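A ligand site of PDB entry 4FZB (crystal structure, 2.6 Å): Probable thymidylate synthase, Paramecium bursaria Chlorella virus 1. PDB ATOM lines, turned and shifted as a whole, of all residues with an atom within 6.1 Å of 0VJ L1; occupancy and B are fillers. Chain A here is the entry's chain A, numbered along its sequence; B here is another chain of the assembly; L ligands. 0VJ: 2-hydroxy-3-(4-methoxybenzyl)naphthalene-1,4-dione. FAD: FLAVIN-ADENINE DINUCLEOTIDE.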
ATOM      1  N   GLU A  91     -19.265  -0.372 -12.573  1.00  0.00           N
ATOM      2  CA  GLU A  91     -18.181   0.058 -13.471  1.00  0.00           C
ATOM      3  C   GLU A  91     -18.216   1.597 -13.582  1.00  0.00           C
ATOM      4  O   GLU A  91     -19.208   2.221 -13.180  1.00  0.00           O
ATOM      5  CB  GLU A  91     -18.325  -0.562 -14.889  1.00  0.00           C
ATOM      6  CG  GLU A  91     -18.730  -2.024 -14.925  1.00  0.00           C
ATOM      7  CD  GLU A  91     -18.878  -2.591 -16.318  1.00  0.00           C
ATOM      8  OE1 GLU A  91     -20.018  -2.880 -16.730  1.00  0.00           O
ATOM      9  OE2 GLU A  91     -17.836  -2.751 -17.002  1.00  0.00           O
ATOM     10  N   PHE A  92     -17.148   2.176 -14.181  1.00  0.00           N
ATOM     11  CA  PHE A  92     -17.056   3.612 -14.426  1.00  0.00           C
ATOM     12  C   PHE A  92     -18.017   4.047 -15.519  1.00  0.00           C
ATOM     13  O   PHE A  92     -18.299   3.268 -16.446  1.00  0.00           O
ATOM     14  CB  PHE A  92     -15.621   4.015 -14.812  1.00  0.00           C
ATOM     15  CG  PHE A  92     -14.682   4.141 -13.637  1.00  0.00           C
ATOM     16  CD1 PHE A  92     -13.647   3.218 -13.459  1.00  0.00           C
ATOM     17  CD2 PHE A  92     -14.822   5.163 -12.701  1.00  0.00           C
ATOM     18  CE1 PHE A  92     -12.781   3.323 -12.368  1.00  0.00           C
ATOM     19  CE2 PHE A  92     -13.970   5.251 -11.600  1.00  0.00           C
ATOM     20  CZ  PHE A  92     -12.951   4.339 -11.447  1.00  0.00           C
ATOM     21  N   SER A  93     -18.516   5.307 -15.420  1.00  0.00           N
ATOM     22  CA  SER A  93     -19.445   5.907 -16.381  1.00  0.00           C
ATOM     23  C   SER A  93     -18.858   5.938 -17.764  1.00  0.00           C
ATOM     24  O   SER A  93     -17.653   6.175 -17.913  1.00  0.00           O
ATOM     25  CB  SER A  93     -19.848   7.314 -15.947  1.00  0.00           C
ATOM     26  OG  SER A  93     -20.915   7.816 -16.741  1.00  0.00           O
ATOM     27  N   GLN A  94     -19.693   5.641 -18.775  1.00  0.00           N
ATOM     28  CA  GLN A  94     -19.252   5.685 -20.171  1.00  0.00           C
ATOM     29  C   GLN A  94     -19.052   7.136 -20.609  1.00  0.00           C
ATOM     30  O   GLN A  94     -18.060   7.439 -21.274  1.00  0.00           O
ATOM     31  CB  GLN A  94     -20.243   4.954 -21.080  1.00  0.00           C
ATOM     32  CG  GLN A  94     -19.711   3.596 -21.554  1.00  0.00           C
ATOM     33  CD  GLN A  94     -20.606   2.442 -21.173  1.00  0.00           C
ATOM     34  OE1 GLN A  94     -20.146   1.295 -21.030  1.00  0.00           O
ATOM     35  NE2 GLN A  94     -21.896   2.695 -21.010  1.00  0.00           N
ATOM     36  N   ARG A  95     -19.945   8.030 -20.159  1.00  0.00           N
ATOM     37  CA  ARG A  95     -19.914   9.453 -20.499  1.00  0.00           C
ATOM     38  C   ARG A  95     -18.879  10.295 -19.721  1.00  0.00           C
ATOM     39  O   ARG A  95     -18.148  11.052 -20.348  1.00  0.00           O
ATOM     40  CB  ARG A  95     -21.300  10.110 -20.384  1.00  0.00           C
ATOM     41  CG  ARG A  95     -22.508   9.169 -20.391  1.00  0.00           C
ATOM     42  CD  ARG A  95     -23.265   9.292 -19.085  1.00  0.00           C
ATOM     43  NE  ARG A  95     -24.560   9.982 -19.228  1.00  0.00           N
ATOM     44  CZ  ARG A  95     -25.542   9.905 -18.336  1.00  0.00           C
ATOM     45  NH1 ARG A  95     -25.399   9.192 -17.232  1.00  0.00           N
ATOM     46  NH2 ARG A  95     -26.691  10.542 -18.551  1.00  0.00           N
ATOM     47  N   GLU A 157     -18.272   8.471 -24.564  1.00  0.00           N
ATOM     48  CA  GLU A 157     -19.045   7.278 -24.980  1.00  0.00           C
ATOM     49  C   GLU A 157     -18.798   6.943 -26.440  1.00  0.00           C
ATOM     50  O   GLU A 157     -18.801   5.768 -26.775  1.00  0.00           O
ATOM     51  CB  GLU A 157     -20.555   7.396 -24.745  1.00  0.00           C
ATOM     52  CG  GLU A 157     -21.007   8.426 -23.740  1.00  0.00           C
ATOM     53  CD  GLU A 157     -21.179   9.820 -24.303  1.00  0.00           C
ATOM     54  OE1 GLU A 157     -20.728  10.775 -23.637  1.00  0.00           O
ATOM     55  OE2 GLU A 157     -21.764   9.957 -25.409  1.00  0.00           O
ATOM     56  N   ALA B  79     -21.750  -4.478 -23.744  1.00  0.00           N
ATOM     57  CA  ALA B  79     -21.252  -4.181 -22.404  1.00  0.00           C
ATOM     58  C   ALA B  79     -22.393  -3.662 -21.472  1.00  0.00           C
ATOM     59  O   ALA B  79     -22.515  -4.149 -20.348  1.00  0.00           O
ATOM     60  CB  ALA B  79     -20.149  -3.134 -22.493  1.00  0.00           C
ATOM     61  N   GLN B  80     -23.227  -2.711 -21.979  1.00  0.00           N
ATOM     62  CA  GLN B  80     -24.401  -2.165 -21.266  1.00  0.00           C
ATOM     63  C   GLN B  80     -25.479  -3.242 -21.202  1.00  0.00           C
ATOM     64  O   GLN B  80     -25.949  -3.546 -20.113  1.00  0.00           O
ATOM     65  CB  GLN B  80     -24.975  -0.903 -21.957  1.00  0.00           C
ATOM     66  CG  GLN B  80     -24.232   0.378 -21.659  1.00  0.00           C
ATOM     67  CD  GLN B  80     -24.280   1.336 -22.828  1.00  0.00           C
ATOM     68  OE1 GLN B  80     -25.301   2.001 -23.099  1.00  0.00           O
ATOM     69  NE2 GLN B  80     -23.153   1.420 -23.542  1.00  0.00           N
ATOM     70  N   ARG B  83     -25.527  -5.917 -18.554  1.00  0.00           N
ATOM     71  CA  ARG B  83     -25.832  -5.441 -17.191  1.00  0.00           C
ATOM     72  C   ARG B  83     -27.296  -5.646 -16.787  1.00  0.00           C
ATOM     73  O   ARG B  83     -27.641  -5.476 -15.613  1.00  0.00           O
ATOM     74  CB  ARG B  83     -25.364  -3.986 -17.002  1.00  0.00           C
ATOM     75  CG  ARG B  83     -23.854  -3.770 -17.254  1.00  0.00           C
ATOM     76  CD  ARG B  83     -22.950  -4.318 -16.134  1.00  0.00           C
ATOM     77  NE  ARG B  83     -23.431  -3.817 -14.849  1.00  0.00           N
ATOM     78  CZ  ARG B  83     -23.133  -2.625 -14.337  1.00  0.00           C
ATOM     79  NH1 ARG B  83     -22.235  -1.850 -14.927  1.00  0.00           N
ATOM     80  NH2 ARG B  83     -23.697  -2.217 -13.215  1.00  0.00           N
ATOM     81  N   HIS B  84     -28.153  -6.053 -17.738  1.00  0.00           N
ATOM     82  CA  HIS B  84     -29.548  -6.306 -17.439  1.00  0.00           C
ATOM     83  C   HIS B  84     -29.632  -7.691 -16.906  1.00  0.00           C
ATOM     84  O   HIS B  84     -29.978  -8.627 -17.646  1.00  0.00           O
ATOM     85  CB  HIS B  84     -30.421  -6.099 -18.669  1.00  0.00           C
ATOM     86  CG  HIS B  84     -30.561  -4.648 -18.980  1.00  0.00           C
ATOM     87  ND1 HIS B  84     -31.473  -3.858 -18.308  1.00  0.00           N
ATOM     88  CD2 HIS B  84     -29.881  -3.884 -19.859  1.00  0.00           C
ATOM     89  CE1 HIS B  84     -31.323  -2.651 -18.810  1.00  0.00           C
ATOM     90  NE2 HIS B  84     -30.390  -2.621 -19.756  1.00  0.00           N
ATOM     91  N   ARG B 187     -34.457   1.667 -22.082  1.00  0.00           N
ATOM     92  CA  ARG B 187     -33.578   1.948 -23.204  1.00  0.00           C
ATOM     93  C   ARG B 187     -34.140   2.741 -24.396  1.00  0.00           C
ATOM     94  O   ARG B 187     -33.384   3.025 -25.326  1.00  0.00           O
ATOM     95  CB  ARG B 187     -32.737   0.739 -23.544  1.00  0.00           C
ATOM     96  CG  ARG B 187     -32.056   0.152 -22.306  1.00  0.00           C
ATOM     97  CD  ARG B 187     -30.886   0.962 -21.782  1.00  0.00           C
ATOM     98  NE  ARG B 187     -29.989   0.067 -21.031  1.00  0.00           N
ATOM     99  CZ  ARG B 187     -28.938   0.458 -20.313  1.00  0.00           C
ATOM    100  NH1 ARG B 187     -28.629   1.744 -20.226  1.00  0.00           N
ATOM    101  NH2 ARG B 187     -28.186  -0.430 -19.694  1.00  0.00           N
ATOM    102  N   GLY B 191     -32.274  10.470 -23.533  1.00  0.00           N
ATOM    103  CA  GLY B 191     -30.926  10.541 -22.964  1.00  0.00           C
ATOM    104  C   GLY B 191     -30.032   9.335 -23.125  1.00  0.00           C
ATOM    105  O   GLY B 191     -28.809   9.467 -23.009  1.00  0.00           O
ATOM    106  N   THR B 192     -30.607   8.157 -23.351  1.00  0.00           N
ATOM    107  CA  THR B 192     -29.810   6.935 -23.482  1.00  0.00           C
ATOM    108  C   THR B 192     -29.021   6.975 -24.784  1.00  0.00           C
ATOM    109  O   THR B 192     -29.479   7.575 -25.756  1.00  0.00           O
ATOM    110  CB  THR B 192     -30.700   5.676 -23.290  1.00  0.00           C
ATOM    111  OG1 THR B 192     -32.005   5.940 -23.791  1.00  0.00           O
ATOM    112  CG2 THR B 192     -30.838   5.263 -21.813  1.00  0.00           C
ATOM    113  N   GLN B 193     -27.805   6.386 -24.785  1.00  0.00           N
ATOM    114  CA  GLN B 193     -26.914   6.269 -25.942  1.00  0.00           C
ATOM    115  C   GLN B 193     -27.693   5.840 -27.194  1.00  0.00           C
ATOM    116  O   GLN B 193     -28.558   4.962 -27.099  1.00  0.00           O
ATOM    117  CB  GLN B 193     -25.784   5.265 -25.660  1.00  0.00           C
ATOM    118  CG  GLN B 193     -24.635   5.359 -26.643  1.00  0.00           C
ATOM    119  CD  GLN B 193     -23.328   4.882 -26.062  1.00  0.00           C
ATOM    120  OE1 GLN B 193     -23.245   4.390 -24.927  1.00  0.00           O
ATOM    121  NE2 GLN B 193     -22.261   5.013 -26.834  1.00  0.00           N
ATOM    122  N   ARG B 194     -27.404   6.468 -28.354  1.00  0.00           N
ATOM    123  CA  ARG B 194     -28.136   6.191 -29.578  1.00  0.00           C
ATOM    124  C   ARG B 194     -27.981   4.817 -30.144  1.00  0.00           C
ATOM    125  O   ARG B 194     -28.974   4.261 -30.611  1.00  0.00           O
ATOM    126  CB  ARG B 194     -27.968   7.291 -30.644  1.00  0.00           C
ATOM    127  CG  ARG B 194     -29.262   7.517 -31.424  1.00  0.00           C
ATOM    128  CD  ARG B 194     -29.171   7.049 -32.860  1.00  0.00           C
ATOM    129  NE  ARG B 194     -29.323   8.179 -33.775  1.00  0.00           N
ATOM    130  CZ  ARG B 194     -29.288   8.106 -35.102  1.00  0.00           C
ATOM    131  NH1 ARG B 194     -29.432   9.205 -35.837  1.00  0.00           N
ATOM    132  NH2 ARG B 194     -29.097   6.942 -35.706  1.00  0.00           N
ATOM    133  N   HIS B 196     -27.884   2.191 -28.646  1.00  0.00           N
ATOM    134  CA  HIS B 196     -28.742   1.445 -27.718  1.00  0.00           C
ATOM    135  C   HIS B 196     -30.231   1.771 -27.880  1.00  0.00           C
ATOM    136  O   HIS B 196     -31.045   0.875 -27.748  1.00  0.00           O
ATOM    137  CB  HIS B 196     -28.329   1.685 -26.266  1.00  0.00           C
ATOM    138  CG  HIS B 196     -28.549   0.491 -25.371  1.00  0.00           C
ATOM    139  ND1 HIS B 196     -27.583   0.074 -24.477  1.00  0.00           N
ATOM    140  CD2 HIS B 196     -29.634  -0.323 -25.267  1.00  0.00           C
ATOM    141  CE1 HIS B 196     -28.096  -0.977 -23.865  1.00  0.00           C
ATOM    142  NE2 HIS B 196     -29.331  -1.252 -24.303  1.00  0.00           N
HETATM  143  C01 0VJ L   1     -21.163   1.164 -17.227  1.00  0.00           C
HETATM  144  C02 0VJ L   1     -22.211  -0.010 -17.548  1.00  0.00           C
HETATM  145  C03 0VJ L   1     -23.495   0.278 -18.047  1.00  0.00           C
HETATM  146  C04 0VJ L   1     -23.819   1.759 -18.240  1.00  0.00           C
HETATM  147  C05 0VJ L   1     -22.906   2.794 -17.987  1.00  0.00           C
HETATM  148  C06 0VJ L   1     -21.540   2.480 -17.483  1.00  0.00           C
HETATM  149  C07 0VJ L   1     -25.261   2.196 -18.746  1.00  0.00           C
HETATM  150  C08 0VJ L   1     -25.622   3.672 -18.942  1.00  0.00           C
HETATM  151  C09 0VJ L   1     -24.656   4.578 -18.651  1.00  0.00           C
HETATM  152  C10 0VJ L   1     -23.263   4.279 -18.182  1.00  0.00           C
HETATM  153  C11 0VJ L   1     -25.054   6.056 -18.827  1.00  0.00           C
HETATM  154  C12 0VJ L   1     -24.828   6.378 -20.181  1.00  0.00           C
HETATM  155  C13 0VJ L   1     -25.739   7.347 -20.441  1.00  0.00           C
HETATM  156  C14 0VJ L   1     -25.691   7.930 -21.755  1.00  0.00           C
HETATM  157  C15 0VJ L   1     -24.779   7.510 -22.806  1.00  0.00           C
HETATM  158  C16 0VJ L   1     -23.809   6.465 -22.581  1.00  0.00           C
HETATM  159  C17 0VJ L   1     -23.797   5.840 -21.240  1.00  0.00           C
HETATM  160  O01 0VJ L   1     -24.916   8.199 -24.121  1.00  0.00           O
HETATM  161  O02 0VJ L   1     -22.487   5.246 -17.955  1.00  0.00           O
HETATM  162  O03 0VJ L   1     -26.086   1.430 -18.917  1.00  0.00           O
HETATM  163  O   0VJ L   1     -26.966   4.091 -19.402  1.00  0.00           O
HETATM  164  C   0VJ L   1     -24.886   9.620 -24.237  1.00  0.00           C
HETATM  165  PA  FAD L   2     -32.825  -5.338 -15.464  1.00  0.00           P
HETATM  166  O1A FAD L   2     -32.337  -6.788 -15.515  1.00  0.00           O
HETATM  167  O2A FAD L   2     -33.412  -4.633 -16.727  1.00  0.00           O
HETATM  168  O5B FAD L   2     -33.904  -5.229 -14.284  1.00  0.00           O
HETATM  169  C5B FAD L   2     -33.684  -6.050 -13.132  1.00  0.00           C
HETATM  170  C4B FAD L   2     -35.034  -6.495 -12.587  1.00  0.00           C
HETATM  171  O4B FAD L   2     -35.752  -5.365 -12.096  1.00  0.00           O
HETATM  172  C3B FAD L   2     -35.970  -7.181 -13.582  1.00  0.00           C
HETATM  173  O3B FAD L   2     -36.435  -8.418 -12.979  1.00  0.00           O
HETATM  174  C2B FAD L   2     -37.010  -6.106 -13.942  1.00  0.00           C
HETATM  175  O2B FAD L   2     -38.297  -6.560 -14.362  1.00  0.00           O
HETATM  176  C1B FAD L   2     -37.105  -5.395 -12.631  1.00  0.00           C
HETATM  177  N9A FAD L   2     -37.519  -4.028 -12.823  1.00  0.00           N
HETATM  178  C8A FAD L   2     -36.724  -3.036 -13.371  1.00  0.00           C
HETATM  179  N7A FAD L   2     -37.370  -1.932 -13.416  1.00  0.00           N
HETATM  180  C5A FAD L   2     -38.620  -2.177 -12.874  1.00  0.00           C
HETATM  181  C6A FAD L   2     -39.754  -1.344 -12.626  1.00  0.00           C
HETATM  182  N6A FAD L   2     -39.743  -0.013 -12.953  1.00  0.00           N
HETATM  183  N1A FAD L   2     -40.925  -1.891 -12.003  1.00  0.00           N
HETATM  184  C2A FAD L   2     -40.921  -3.259 -11.690  1.00  0.00           C
HETATM  185  N3A FAD L   2     -39.851  -4.080 -11.908  1.00  0.00           N
HETATM  186  C4A FAD L   2     -38.749  -3.486 -12.490  1.00  0.00           C
HETATM  187  N1  FAD L   2     -23.687   1.408 -14.269  1.00  0.00           N
HETATM  188  C2  FAD L   2     -22.416   1.539 -13.793  1.00  0.00           C
HETATM  189  O2  FAD L   2     -21.841   0.496 -13.438  1.00  0.00           O
HETATM  190  N3  FAD L   2     -21.831   2.799 -13.824  1.00  0.00           N
HETATM  191  C4  FAD L   2     -22.451   3.990 -14.213  1.00  0.00           C
HETATM  192  O4  FAD L   2     -21.860   5.078 -14.228  1.00  0.00           O
HETATM  193  C4X FAD L   2     -23.918   3.846 -14.687  1.00  0.00           C
HETATM  194  N5  FAD L   2     -24.663   4.874 -15.089  1.00  0.00           N
HETATM  195  C5X FAD L   2     -25.993   4.565 -15.535  1.00  0.00           C
HETATM  196  C6  FAD L   2     -26.813   5.658 -15.933  1.00  0.00           C
HETATM  197  C7  FAD L   2     -28.154   5.479 -16.395  1.00  0.00           C
HETATM  198  C7M FAD L   2     -28.954   6.715 -16.770  1.00  0.00           C
HETATM  199  C8  FAD L   2     -28.706   4.145 -16.477  1.00  0.00           C
HETATM  200  C8M FAD L   2     -30.101   3.836 -16.949  1.00  0.00           C
HETATM  201  C9  FAD L   2     -27.900   3.060 -16.094  1.00  0.00           C
HETATM  202  C9A FAD L   2     -26.551   3.211 -15.611  1.00  0.00           C
HETATM  203  N10 FAD L   2     -25.764   2.114 -15.173  1.00  0.00           N
HETATM  204  C10 FAD L   2     -24.461   2.387 -14.699  1.00  0.00           C
HETATM  205  C1' FAD L   2     -26.276   0.722 -15.206  1.00  0.00           C
HETATM  206  C2' FAD L   2     -27.391   0.535 -14.150  1.00  0.00           C
HETATM  207  O2' FAD L   2     -26.882   0.799 -12.843  1.00  0.00           O
HETATM  208  C3' FAD L   2     -28.055  -0.865 -14.127  1.00  0.00           C
HETATM  209  O3' FAD L   2     -27.291  -1.771 -13.356  1.00  0.00           O
HETATM  210  C4' FAD L   2     -28.399  -1.506 -15.480  1.00  0.00           C
HETATM  211  O4' FAD L   2     -29.266  -0.526 -16.078  1.00  0.00           O
HETATM  212  C5' FAD L   2     -29.200  -2.813 -15.302  1.00  0.00           C
HETATM  213  O5' FAD L   2     -30.527  -2.448 -14.758  1.00  0.00           O
HETATM  214  P   FAD L   2     -31.354  -3.409 -13.757  1.00  0.00           P
HETATM  215  O1P FAD L   2     -30.354  -4.029 -12.798  1.00  0.00           O
HETATM  216  O2P FAD L   2     -32.614  -2.685 -13.294  1.00  0.00           O
HETATM  217  O3P FAD L   2     -31.615  -4.476 -14.883  1.00  0.00           O
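N of Glu 91 sits at hydrogen-bond distance from O2 of FAD L2 (2.9 Å). An oxygen (O02) of 0VJ L1 sits at hydrogen-bond distance from the side-chain hydroxyl of Ser 93, at 3.2 Å. ND1 of His 84 of chain B is in hydrogen-bond range of O2A of FAD L2, 2.6 Å away. N of Gln 94 lies within hydrogen-bond range of O02 of 0VJ L1 (2.9 Å). N of Gln 193 of chain B sits close to O01 of 0VJ L1 (3.5 Å). The guanidinium group (NH1) of Arg 83 of chain B sits at hydrogen-bond distance from an oxygen (O2) of FAD L2, at 2.8 Å. The guanidinium group (NH1) of Arg 187 of chain B is in hydrogen-bond range of an oxygen (O03) of 0VJ L1 (2.9 Å). O of Glu 91 is in hydrogen-bond range of N3 of FAD L2, at 2.8 Å.
OE1 of Glu 91 is in salt-bridge range of NH1 of Arg 83 of chain B, 3.0 Å away. NE2 of Gln 94 sits close to NE2 of Gln 80 of chain B, 3.1 Å away. The backbone carbonyl oxygen (O) of Gln 94 sits at hydrogen-bond distance from the backbone NH (N) of Glu 157, 3.5 Å away. OE1 of Gln 80 of chain B is in hydrogen-bond range of ND1 of His 196 of chain B, at 3.3 Å. The guanidinium group (NE) of Arg 187 of chain B lies within hydrogen-bond range of a ring nitrogen (NE2) of His 84 of chain B (3.0 Å). NE2 of Gln 80 of chain B lies within hydrogen-bond range of OE1 of Gln 193 of chain B (3.3 Å).
Residues that only touch 0VJ L1: Glu 91, Phe 92, Arg 95, Glu 157, Gln 80 of chain B, Arg 83 of chain B and Gly 191 of chain B. Of the 16 residues printed, 11 come within 4 Å of 0VJ L1.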
